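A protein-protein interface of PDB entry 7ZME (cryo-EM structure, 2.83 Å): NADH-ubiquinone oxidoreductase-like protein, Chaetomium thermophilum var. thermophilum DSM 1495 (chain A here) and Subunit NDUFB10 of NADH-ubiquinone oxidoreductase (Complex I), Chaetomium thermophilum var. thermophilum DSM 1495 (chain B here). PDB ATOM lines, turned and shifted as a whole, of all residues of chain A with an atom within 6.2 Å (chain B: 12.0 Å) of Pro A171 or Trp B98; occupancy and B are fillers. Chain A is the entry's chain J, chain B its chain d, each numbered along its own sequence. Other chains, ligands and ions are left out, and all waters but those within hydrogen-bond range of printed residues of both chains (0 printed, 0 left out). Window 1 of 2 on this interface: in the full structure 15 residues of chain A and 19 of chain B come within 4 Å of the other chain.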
ATOM      1  N   ARG A 152     -18.570 -32.563   1.997  1.00  0.00           N
ATOM      2  CA  ARG A 152     -19.164 -31.706   3.014  1.00  0.00           C
ATOM      3  C   ARG A 152     -18.636 -32.115   4.378  1.00  0.00           C
ATOM      4  O   ARG A 152     -18.723 -33.286   4.757  1.00  0.00           O
ATOM      5  CB  ARG A 152     -20.686 -31.796   3.003  1.00  0.00           C
ATOM      6  CG  ARG A 152     -21.321 -31.254   1.761  1.00  0.00           C
ATOM      7  CD  ARG A 152     -22.825 -31.418   1.785  1.00  0.00           C
ATOM      8  NE  ARG A 152     -23.474 -30.643   2.835  1.00  0.00           N
ATOM      9  CZ  ARG A 152     -23.863 -29.383   2.684  1.00  0.00           C
ATOM     10  NH1 ARG A 152     -23.634 -28.760   1.542  1.00  0.00           N
ATOM     11  NH2 ARG A 152     -24.461 -28.737   3.671  1.00  0.00           N
ATOM     12  N   ILE A 155     -19.964 -28.127  10.068  1.00  0.00           N
ATOM     13  CA  ILE A 155     -19.599 -26.723  10.177  1.00  0.00           C
ATOM     14  C   ILE A 155     -18.675 -26.480  11.359  1.00  0.00           C
ATOM     15  O   ILE A 155     -17.913 -25.511  11.358  1.00  0.00           O
ATOM     16  CB  ILE A 155     -20.862 -25.844  10.255  1.00  0.00           C
ATOM     17  CG1 ILE A 155     -20.537 -24.414   9.820  1.00  0.00           C
ATOM     18  CG2 ILE A 155     -21.450 -25.865  11.652  1.00  0.00           C
ATOM     19  CD1 ILE A 155     -21.730 -23.504   9.756  1.00  0.00           C
ATOM     20  N   GLU A 164     -15.000 -17.475  13.570  1.00  0.00           N
ATOM     21  CA  GLU A 164     -16.349 -17.007  13.291  1.00  0.00           C
ATOM     22  C   GLU A 164     -16.303 -15.503  13.074  1.00  0.00           C
ATOM     23  O   GLU A 164     -15.756 -14.770  13.905  1.00  0.00           O
ATOM     24  CB  GLU A 164     -17.291 -17.362  14.438  1.00  0.00           C
ATOM     25  CG  GLU A 164     -18.729 -17.009  14.186  1.00  0.00           C
ATOM     26  CD  GLU A 164     -19.642 -17.475  15.299  1.00  0.00           C
ATOM     27  OE1 GLU A 164     -19.131 -18.015  16.302  1.00  0.00           O
ATOM     28  OE2 GLU A 164     -20.872 -17.313  15.166  1.00  0.00           O
ATOM     29  N   LYS A 169     -20.714 -15.982   9.194  1.00  0.00           N
ATOM     30  CA  LYS A 169     -21.767 -15.581  10.122  1.00  0.00           C
ATOM     31  C   LYS A 169     -22.784 -16.710  10.159  1.00  0.00           C
ATOM     32  O   LYS A 169     -23.834 -16.640   9.507  1.00  0.00           O
ATOM     33  CB  LYS A 169     -22.401 -14.262   9.682  1.00  0.00           C
ATOM     34  CG  LYS A 169     -21.583 -13.018   9.999  1.00  0.00           C
ATOM     35  CD  LYS A 169     -22.472 -11.791  10.105  1.00  0.00           C
ATOM     36  CE  LYS A 169     -21.694 -10.566  10.561  1.00  0.00           C
ATOM     37  NZ  LYS A 169     -22.362  -9.846  11.678  1.00  0.00           N
ATOM     38  N   PRO A 170     -22.499 -17.777  10.898  1.00  0.00           N
ATOM     39  CA  PRO A 170     -23.397 -18.932  10.925  1.00  0.00           C
ATOM     40  C   PRO A 170     -24.673 -18.592  11.672  1.00  0.00           C
ATOM     41  O   PRO A 170     -24.723 -17.579  12.383  1.00  0.00           O
ATOM     42  CB  PRO A 170     -22.574 -19.997  11.672  1.00  0.00           C
ATOM     43  CG  PRO A 170     -21.185 -19.441  11.770  1.00  0.00           C
ATOM     44  CD  PRO A 170     -21.338 -17.970  11.777  1.00  0.00           C
ATOM     45  N   PRO A 171     -25.732 -19.390  11.533  1.00  0.00           N
ATOM     46  CA  PRO A 171     -26.958 -19.082  12.277  1.00  0.00           C
ATOM     47  C   PRO A 171     -26.707 -19.096  13.776  1.00  0.00           C
ATOM     48  O   PRO A 171     -26.002 -19.959  14.302  1.00  0.00           O
ATOM     49  CB  PRO A 171     -27.935 -20.185  11.842  1.00  0.00           C
ATOM     50  CG  PRO A 171     -27.215 -20.993  10.797  1.00  0.00           C
ATOM     51  CD  PRO A 171     -25.769 -20.747  10.967  1.00  0.00           C
ATOM     52  N   GLY A 172     -27.293 -18.118  14.462  1.00  0.00           N
ATOM     53  CA  GLY A 172     -26.992 -17.886  15.858  1.00  0.00           C
ATOM     54  C   GLY A 172     -25.776 -17.026  16.113  1.00  0.00           C
ATOM     55  O   GLY A 172     -25.349 -16.911  17.266  1.00  0.00           O
ATOM     56  N   TYR A 173     -25.199 -16.424  15.069  1.00  0.00           N
ATOM     57  CA  TYR A 173     -24.021 -15.579  15.242  1.00  0.00           C
ATOM     58  C   TYR A 173     -24.339 -14.347  16.075  1.00  0.00           C
ATOM     59  O   TYR A 173     -23.557 -13.962  16.952  1.00  0.00           O
ATOM     60  CB  TYR A 173     -23.471 -15.167  13.875  1.00  0.00           C
ATOM     61  CG  TYR A 173     -22.381 -14.118  13.932  1.00  0.00           C
ATOM     62  CD1 TYR A 173     -21.051 -14.482  14.055  1.00  0.00           C
ATOM     63  CD2 TYR A 173     -22.683 -12.767  13.866  1.00  0.00           C
ATOM     64  CE1 TYR A 173     -20.059 -13.541  14.113  1.00  0.00           C
ATOM     65  CE2 TYR A 173     -21.695 -11.821  13.930  1.00  0.00           C
ATOM     66  CZ  TYR A 173     -20.384 -12.211  14.048  1.00  0.00           C
ATOM     67  OH  TYR A 173     -19.389 -11.260  14.103  1.00  0.00           O
ATOM     68  N   TYR A 174     -25.477 -13.706  15.809  1.00  0.00           N
ATOM     69  CA  TYR A 174     -25.777 -12.427  16.441  1.00  0.00           C
ATOM     70  C   TYR A 174     -26.010 -12.583  17.938  1.00  0.00           C
ATOM     71  O   TYR A 174     -25.578 -11.737  18.729  1.00  0.00           O
ATOM     72  CB  TYR A 174     -26.990 -11.789  15.767  1.00  0.00           C
ATOM     73  CG  TYR A 174     -26.657 -11.066  14.482  1.00  0.00           C
ATOM     74  CD1 TYR A 174     -25.714 -10.049  14.459  1.00  0.00           C
ATOM     75  CD2 TYR A 174     -27.285 -11.405  13.292  1.00  0.00           C
ATOM     76  CE1 TYR A 174     -25.406  -9.386  13.285  1.00  0.00           C
ATOM     77  CE2 TYR A 174     -26.985 -10.750  12.114  1.00  0.00           C
ATOM     78  CZ  TYR A 174     -26.045  -9.741  12.116  1.00  0.00           C
ATOM     79  OH  TYR A 174     -25.744  -9.086  10.943  1.00  0.00           O
ATOM     80  N   ARG A 176     -24.672 -14.915  19.800  1.00  0.00           N
ATOM     81  CA  ARG A 176     -23.349 -15.158  20.367  1.00  0.00           C
ATOM     82  C   ARG A 176     -22.561 -13.863  20.485  1.00  0.00           C
ATOM     83  O   ARG A 176     -21.825 -13.659  21.458  1.00  0.00           O
ATOM     84  CB  ARG A 176     -22.587 -16.166  19.509  1.00  0.00           C
ATOM     85  CG  ARG A 176     -22.658 -17.593  20.005  1.00  0.00           C
ATOM     86  CD  ARG A 176     -22.084 -18.538  18.972  1.00  0.00           C
ATOM     87  NE  ARG A 176     -22.722 -18.365  17.673  1.00  0.00           N
ATOM     88  CZ  ARG A 176     -22.741 -19.292  16.723  1.00  0.00           C
ATOM     89  NH1 ARG A 176     -23.346 -19.049  15.569  1.00  0.00           N
ATOM     90  NH2 ARG A 176     -22.152 -20.462  16.927  1.00  0.00           N
ATOM     91  N   PRO B  18     -33.573 -23.900  -2.778  1.00  0.00           N
ATOM     92  CA  PRO B  18     -32.175 -23.485  -2.555  1.00  0.00           C
ATOM     93  C   PRO B  18     -31.557 -24.149  -1.327  1.00  0.00           C
ATOM     94  O   PRO B  18     -31.398 -23.569  -0.256  1.00  0.00           O
ATOM     95  CB  PRO B  18     -32.298 -21.968  -2.380  1.00  0.00           C
ATOM     96  CG  PRO B  18     -33.748 -21.629  -2.672  1.00  0.00           C
ATOM     97  CD  PRO B  18     -34.506 -22.856  -2.343  1.00  0.00           C
ATOM     98  N   THR B  19     -31.202 -25.420  -1.483  1.00  0.00           N
ATOM     99  CA  THR B  19     -30.580 -26.180  -0.413  1.00  0.00           C
ATOM    100  C   THR B  19     -29.508 -27.085  -1.000  1.00  0.00           C
ATOM    101  O   THR B  19     -29.519 -27.409  -2.189  1.00  0.00           O
ATOM    102  CB  THR B  19     -31.612 -27.010   0.368  1.00  0.00           C
ATOM    103  OG1 THR B  19     -31.053 -27.431   1.616  1.00  0.00           O
ATOM    104  CG2 THR B  19     -32.036 -28.231  -0.429  1.00  0.00           C
ATOM    105  N   PHE B  20     -28.557 -27.470  -0.153  1.00  0.00           N
ATOM    106  CA  PHE B  20     -27.599 -28.518  -0.477  1.00  0.00           C
ATOM    107  C   PHE B  20     -27.899 -29.804   0.281  1.00  0.00           C
ATOM    108  O   PHE B  20     -27.038 -30.683   0.376  1.00  0.00           O
ATOM    109  CB  PHE B  20     -26.172 -28.051  -0.190  1.00  0.00           C
ATOM    110  CG  PHE B  20     -25.602 -27.169  -1.256  1.00  0.00           C
ATOM    111  CD1 PHE B  20     -25.252 -27.691  -2.486  1.00  0.00           C
ATOM    112  CD2 PHE B  20     -25.424 -25.820  -1.031  1.00  0.00           C
ATOM    113  CE1 PHE B  20     -24.736 -26.885  -3.469  1.00  0.00           C
ATOM    114  CE2 PHE B  20     -24.907 -25.009  -2.010  1.00  0.00           C
ATOM    115  CZ  PHE B  20     -24.562 -25.543  -3.233  1.00  0.00           C
ATOM    116  N   ASP B  21     -29.099 -29.919   0.839  1.00  0.00           N
ATOM    117  CA  ASP B  21     -29.491 -31.084   1.615  1.00  0.00           C
ATOM    118  C   ASP B  21     -30.152 -32.109   0.707  1.00  0.00           C
ATOM    119  O   ASP B  21     -31.023 -31.765  -0.100  1.00  0.00           O
ATOM    120  CB  ASP B  21     -30.441 -30.682   2.744  1.00  0.00           C
ATOM    121  CG  ASP B  21     -29.756 -29.861   3.816  1.00  0.00           C
ATOM    122  OD1 ASP B  21     -28.536 -30.043   4.018  1.00  0.00           O
ATOM    123  OD2 ASP B  21     -30.436 -29.036   4.460  1.00  0.00           O
ATOM    124  N   GLY B  22     -29.734 -33.364   0.836  1.00  0.00           N
ATOM    125  CA  GLY B  22     -30.296 -34.419   0.014  1.00  0.00           C
ATOM    126  C   GLY B  22     -29.911 -34.327  -1.444  1.00  0.00           C
ATOM    127  O   GLY B  22     -30.639 -34.836  -2.303  1.00  0.00           O
ATOM    128  N   TYR B  25     -23.724 -34.849  -4.912  1.00  0.00           N
ATOM    129  CA  TYR B  25     -22.739 -34.050  -5.630  1.00  0.00           C
ATOM    130  C   TYR B  25     -22.207 -34.773  -6.861  1.00  0.00           C
ATOM    131  O   TYR B  25     -21.621 -34.132  -7.740  1.00  0.00           O
ATOM    132  CB  TYR B  25     -21.581 -33.660  -4.704  1.00  0.00           C
ATOM    133  CG  TYR B  25     -21.911 -32.607  -3.659  1.00  0.00           C
ATOM    134  CD1 TYR B  25     -23.222 -32.291  -3.342  1.00  0.00           C
ATOM    135  CD2 TYR B  25     -20.901 -31.930  -2.992  1.00  0.00           C
ATOM    136  CE1 TYR B  25     -23.517 -31.339  -2.392  1.00  0.00           C
ATOM    137  CE2 TYR B  25     -21.189 -30.974  -2.038  1.00  0.00           C
ATOM    138  CZ  TYR B  25     -22.501 -30.682  -1.744  1.00  0.00           C
ATOM    139  OH  TYR B  25     -22.800 -29.729  -0.802  1.00  0.00           O
ATOM    140  N   ILE B  38     -29.380 -21.214  -4.822  1.00  0.00           N
ATOM    141  CA  ILE B  38     -28.816 -20.462  -3.704  1.00  0.00           C
ATOM    142  C   ILE B  38     -28.506 -19.032  -4.129  1.00  0.00           C
ATOM    143  O   ILE B  38     -28.795 -18.074  -3.403  1.00  0.00           O
ATOM    144  CB  ILE B  38     -27.563 -21.181  -3.166  1.00  0.00           C
ATOM    145  CG1 ILE B  38     -27.963 -22.414  -2.360  1.00  0.00           C
ATOM    146  CG2 ILE B  38     -26.726 -20.253  -2.307  1.00  0.00           C
ATOM    147  CD1 ILE B  38     -28.761 -22.088  -1.131  1.00  0.00           C
ATOM    148  N   GLN B  42     -30.335 -15.215  -2.903  1.00  0.00           N
ATOM    149  CA  GLN B  42     -29.534 -14.139  -2.334  1.00  0.00           C
ATOM    150  C   GLN B  42     -29.680 -12.859  -3.142  1.00  0.00           C
ATOM    151  O   GLN B  42     -29.782 -11.764  -2.575  1.00  0.00           O
ATOM    152  CB  GLN B  42     -28.069 -14.559  -2.279  1.00  0.00           C
ATOM    153  CG  GLN B  42     -27.689 -15.371  -1.074  1.00  0.00           C
ATOM    154  CD  GLN B  42     -26.329 -15.993  -1.231  1.00  0.00           C
ATOM    155  OE1 GLN B  42     -25.757 -16.005  -2.319  1.00  0.00           O
ATOM    156  NE2 GLN B  42     -25.794 -16.513  -0.138  1.00  0.00           N
ATOM    157  N   ALA B  83     -29.309  -5.340   6.767  1.00  0.00           N
ATOM    158  CA  ALA B  83     -28.592  -6.161   7.733  1.00  0.00           C
ATOM    159  C   ALA B  83     -28.656  -7.650   7.426  1.00  0.00           C
ATOM    160  O   ALA B  83     -27.874  -8.413   8.000  1.00  0.00           O
ATOM    161  CB  ALA B  83     -29.136  -5.911   9.138  1.00  0.00           C
ATOM    162  N   ASN B  84     -29.550  -8.083   6.544  1.00  0.00           N
ATOM    163  CA  ASN B  84     -29.720  -9.497   6.237  1.00  0.00           C
ATOM    164  C   ASN B  84     -29.321  -9.871   4.821  1.00  0.00           C
ATOM    165  O   ASN B  84     -28.634 -10.873   4.625  1.00  0.00           O
ATOM    166  CB  ASN B  84     -31.173  -9.919   6.472  1.00  0.00           C
ATOM    167  CG  ASN B  84     -31.588  -9.791   7.920  1.00  0.00           C
ATOM    168  OD1 ASN B  84     -32.449  -8.984   8.261  1.00  0.00           O
ATOM    169  ND2 ASN B  84     -30.968 -10.584   8.784  1.00  0.00           N
ATOM    170  N   LYS B  88     -23.484 -13.813  -0.755  1.00  0.00           N
ATOM    171  CA  LYS B  88     -22.365 -14.475  -0.104  1.00  0.00           C
ATOM    172  C   LYS B  88     -21.903 -15.732  -0.822  1.00  0.00           C
ATOM    173  O   LYS B  88     -20.883 -16.304  -0.430  1.00  0.00           O
ATOM    174  CB  LYS B  88     -22.724 -14.832   1.344  1.00  0.00           C
ATOM    175  CG  LYS B  88     -23.016 -13.646   2.230  1.00  0.00           C
ATOM    176  CD  LYS B  88     -21.786 -12.786   2.388  1.00  0.00           C
ATOM    177  CE  LYS B  88     -20.740 -13.476   3.242  1.00  0.00           C
ATOM    178  NZ  LYS B  88     -19.551 -12.614   3.471  1.00  0.00           N
ATOM    179  N   TYR B  90     -22.542 -19.701  -2.797  1.00  0.00           N
ATOM    180  CA  TYR B  90     -22.994 -21.037  -2.441  1.00  0.00           C
ATOM    181  C   TYR B  90     -21.894 -21.873  -1.810  1.00  0.00           C
ATOM    182  O   TYR B  90     -22.159 -22.994  -1.372  1.00  0.00           O
ATOM    183  CB  TYR B  90     -23.537 -21.760  -3.682  1.00  0.00           C
ATOM    184  CG  TYR B  90     -22.530 -21.960  -4.805  1.00  0.00           C
ATOM    185  CD1 TYR B  90     -21.453 -22.826  -4.666  1.00  0.00           C
ATOM    186  CD2 TYR B  90     -22.663 -21.286  -6.002  1.00  0.00           C
ATOM    187  CE1 TYR B  90     -20.542 -23.001  -5.674  1.00  0.00           C
ATOM    188  CE2 TYR B  90     -21.759 -21.466  -7.022  1.00  0.00           C
ATOM    189  CZ  TYR B  90     -20.699 -22.322  -6.851  1.00  0.00           C
ATOM    190  OH  TYR B  90     -19.792 -22.503  -7.865  1.00  0.00           O
ATOM    191  N   LEU B  91     -20.667 -21.360  -1.768  1.00  0.00           N
ATOM    192  CA  LEU B  91     -19.505 -22.197  -1.515  1.00  0.00           C
ATOM    193  C   LEU B  91     -19.392 -22.625  -0.060  1.00  0.00           C
ATOM    194  O   LEU B  91     -18.888 -23.716   0.216  1.00  0.00           O
ATOM    195  CB  LEU B  91     -18.240 -21.458  -1.952  1.00  0.00           C
ATOM    196  CG  LEU B  91     -16.960 -22.268  -2.131  1.00  0.00           C
ATOM    197  CD1 LEU B  91     -17.171 -23.369  -3.150  1.00  0.00           C
ATOM    198  CD2 LEU B  91     -15.838 -21.352  -2.569  1.00  0.00           C
ATOM    199  N   PHE B  92     -19.841 -21.798   0.884  1.00  0.00           N
ATOM    200  CA  PHE B  92     -19.734 -22.188   2.285  1.00  0.00           C
ATOM    201  C   PHE B  92     -20.757 -23.260   2.637  1.00  0.00           C
ATOM    202  O   PHE B  92     -20.446 -24.201   3.373  1.00  0.00           O
ATOM    203  CB  PHE B  92     -19.895 -20.969   3.194  1.00  0.00           C
ATOM    204  CG  PHE B  92     -19.496 -21.226   4.618  1.00  0.00           C
ATOM    205  CD1 PHE B  92     -20.399 -21.753   5.523  1.00  0.00           C
ATOM    206  CD2 PHE B  92     -18.211 -20.958   5.047  1.00  0.00           C
ATOM    207  CE1 PHE B  92     -20.029 -21.998   6.827  1.00  0.00           C
ATOM    208  CE2 PHE B  92     -17.835 -21.204   6.350  1.00  0.00           C
ATOM    209  CZ  PHE B  92     -18.745 -21.722   7.241  1.00  0.00           C
ATOM    210  N   GLU B  93     -21.983 -23.132   2.128  1.00  0.00           N
ATOM    211  CA  GLU B  93     -22.999 -24.143   2.396  1.00  0.00           C
ATOM    212  C   GLU B  93     -22.707 -25.440   1.658  1.00  0.00           C
ATOM    213  O   GLU B  93     -23.041 -26.521   2.155  1.00  0.00           O
ATOM    214  CB  GLU B  93     -24.382 -23.625   2.013  1.00  0.00           C
ATOM    215  CG  GLU B  93     -25.018 -22.731   3.052  1.00  0.00           C
ATOM    216  CD  GLU B  93     -26.475 -22.461   2.760  1.00  0.00           C
ATOM    217  OE1 GLU B  93     -27.250 -23.433   2.660  1.00  0.00           O
ATOM    218  OE2 GLU B  93     -26.846 -21.279   2.619  1.00  0.00           O
ATOM    219  N   GLN B  94     -22.100 -25.357   0.476  1.00  0.00           N
ATOM    220  CA  GLN B  94     -21.774 -26.559  -0.277  1.00  0.00           C
ATOM    221  C   GLN B  94     -20.719 -27.408   0.415  1.00  0.00           C
ATOM    222  O   GLN B  94     -20.596 -28.596   0.104  1.00  0.00           O
ATOM    223  CB  GLN B  94     -21.303 -26.184  -1.679  1.00  0.00           C
ATOM    224  CG  GLN B  94     -21.327 -27.331  -2.665  1.00  0.00           C
ATOM    225  CD  GLN B  94     -20.709 -26.970  -3.987  1.00  0.00           C
ATOM    226  OE1 GLN B  94     -21.187 -26.078  -4.684  1.00  0.00           O
ATOM    227  NE2 GLN B  94     -19.635 -27.659  -4.343  1.00  0.00           N
ATOM    228  N   GLN B  95     -19.960 -26.835   1.346  1.00  0.00           N
ATOM    229  CA  GLN B  95     -18.890 -27.551   2.018  1.00  0.00           C
ATOM    230  C   GLN B  95     -19.138 -27.785   3.500  1.00  0.00           C
ATOM    231  O   GLN B  95     -18.382 -28.538   4.118  1.00  0.00           O
ATOM    232  CB  GLN B  95     -17.561 -26.805   1.837  1.00  0.00           C
ATOM    233  CG  GLN B  95     -17.298 -26.376   0.408  1.00  0.00           C
ATOM    234  CD  GLN B  95     -15.853 -26.017   0.158  1.00  0.00           C
ATOM    235  OE1 GLN B  95     -15.351 -26.165  -0.952  1.00  0.00           O
ATOM    236  NE2 GLN B  95     -15.174 -25.541   1.191  1.00  0.00           N
ATOM    237  N   ASN B  96     -20.160 -27.168   4.084  1.00  0.00           N
ATOM    238  CA  ASN B  96     -20.472 -27.350   5.494  1.00  0.00           C
ATOM    239  C   ASN B  96     -21.965 -27.562   5.662  1.00  0.00           C
ATOM    240  O   ASN B  96     -22.766 -26.959   4.943  1.00  0.00           O
ATOM    241  CB  ASN B  96     -20.020 -26.149   6.335  1.00  0.00           C
ATOM    242  CG  ASN B  96     -18.602 -25.733   6.040  1.00  0.00           C
ATOM    243  OD1 ASN B  96     -17.654 -26.383   6.470  1.00  0.00           O
ATOM    244  ND2 ASN B  96     -18.445 -24.646   5.304  1.00  0.00           N
ATOM    245  N   TYR B  97     -22.339 -28.418   6.611  1.00  0.00           N
ATOM    246  CA  TYR B  97     -23.739 -28.649   6.933  1.00  0.00           C
ATOM    247  C   TYR B  97     -23.980 -28.319   8.398  1.00  0.00           C
ATOM    248  O   TYR B  97     -23.131 -28.581   9.255  1.00  0.00           O
ATOM    249  CB  TYR B  97     -24.169 -30.092   6.647  1.00  0.00           C
ATOM    250  CG  TYR B  97     -23.146 -31.153   6.966  1.00  0.00           C
ATOM    251  CD1 TYR B  97     -22.925 -31.558   8.276  1.00  0.00           C
ATOM    252  CD2 TYR B  97     -22.445 -31.794   5.959  1.00  0.00           C
ATOM    253  CE1 TYR B  97     -22.009 -32.545   8.574  1.00  0.00           C
ATOM    254  CE2 TYR B  97     -21.521 -32.781   6.249  1.00  0.00           C
ATOM    255  CZ  TYR B  97     -21.306 -33.151   7.557  1.00  0.00           C
ATOM    256  OH  TYR B  97     -20.390 -34.135   7.847  1.00  0.00           O
ATOM    257  N   TRP B  98     -25.146 -27.746   8.678  1.00  0.00           N
ATOM    258  CA  TRP B  98     -25.489 -27.266  10.006  1.00  0.00           C
ATOM    259  C   TRP B  98     -26.827 -27.847  10.432  1.00  0.00           C
ATOM    260  O   TRP B  98     -27.760 -27.933   9.628  1.00  0.00           O
ATOM    261  CB  TRP B  98     -25.538 -25.737  10.031  1.00  0.00           C
ATOM    262  CG  TRP B  98     -26.280 -25.172  11.191  1.00  0.00           C
ATOM    263  CD1 TRP B  98     -25.830 -25.049  12.469  1.00  0.00           C
ATOM    264  CD2 TRP B  98     -27.607 -24.637  11.178  1.00  0.00           C
ATOM    265  NE1 TRP B  98     -26.795 -24.475  13.258  1.00  0.00           N
ATOM    266  CE2 TRP B  98     -27.896 -24.212  12.487  1.00  0.00           C
ATOM    267  CE3 TRP B  98     -28.576 -24.477  10.187  1.00  0.00           C
ATOM    268  CZ2 TRP B  98     -29.117 -23.636  12.832  1.00  0.00           C
ATOM    269  CZ3 TRP B  98     -29.786 -23.907  10.529  1.00  0.00           C
ATOM    270  CH2 TRP B  98     -30.047 -23.495  11.841  1.00  0.00           C
ATOM    271  N   SER B  99     -26.907 -28.249  11.699  1.00  0.00           N
ATOM    272  CA  SER B  99     -28.133 -28.779  12.291  1.00  0.00           C
ATOM    273  C   SER B  99     -28.677 -29.972  11.512  1.00  0.00           C
ATOM    274  O   SER B  99     -29.861 -30.294  11.599  1.00  0.00           O
ATOM    275  CB  SER B  99     -29.198 -27.683  12.385  1.00  0.00           C
ATOM    276  OG  SER B  99     -30.410 -28.192  12.914  1.00  0.00           O
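NH1 of Arg A152 lies within hydrogen-bond range of OH of Tyr B25 (2.7 Å).
The backbone carbonyl oxygen of Glu B93 sits close to the guanidinium group of Arg A152, 3.0 Å away.
The guanidinium group (NH1) of Arg A152 sits close to the backbone carbonyl oxygen (O) of Gln B94 (3.4 Å).
The backbone carbonyl oxygen (O) of Asn B96 lies within hydrogen-bond range of the guanidinium group (NH2) of Arg A152 (2.8 Å).
The backbone NH (N) of Ile A155 sits at hydrogen-bond distance from the backbone carbonyl oxygen (O) of Tyr B97, at 3.3 Å.
Arg A152 touches Phe B20 (NH1 to CB, 3.2 Å).
CA of Arg A152 touches O of Gln B95, 3.4 Å away.
Tyr B97 touches Arg A152 (CE2 to O, 3.2 Å).
CE1 of Phe B92 touches CD1 of Ile A155, 3.7 Å away.
CA of Ile A155 touches CB of Asn B96 (3.9 Å).
Pro A171 touches Trp B98 (CG to CD2, 3.7 Å).
Ala B83 touches Tyr A174.
Hydrophobic or aromatic side chains of chain B that line the printed part of chain A: Phe B20, Tyr B25, Phe B92, Tyr B97 and Trp B98.
Printed residues of chain A that touch a printed residue of chain B: Arg A152, Ile A155, Pro A171 and Tyr A174.
Among the printed residues, 12 pairs touch across the chains.
Among the printed residues, no Asp or Glu carboxylate lies within 4 Å of a Lys or Arg side-chain nitrogen of the other chain.
O of Pro A171 is in hydrogen-bond range of NH1 of Arg A176 (3.1 Å).
OH of Tyr B25 sits at hydrogen-bond distance from O of Gln B94 (2.6 Å).
The backbone carbonyl oxygen of Phe B92 sits at hydrogen-bond distance from the side-chain amide nitrogen of Asn B96, at 2.8 Å.
Ile A155 touches just these residues of chain B: Phe B92, Asn B96 and Tyr B97.
No residue of chain B comes within 4 Å of Pro A170.
Pro A171 touches just one residue of chain B: Trp B98.
Gly A172 touches none of the printed residues of chain B.
Of the printed residues of chain A, Ala B83 touches Tyr A174 (3.7 Å).
Printed residues of chain A within 4 Å of Gln B95: Arg A152 (3.4 Å).
Of chain A, only Pro A171 comes within 4 Å of Trp B98.
The nearest residue of chain B that does not touch Pro A171 is Ser B99 (7.2 Å).
The nearest printed residue of chain A that does not touch Ala B83 is Lys A169 (6.7 Å).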
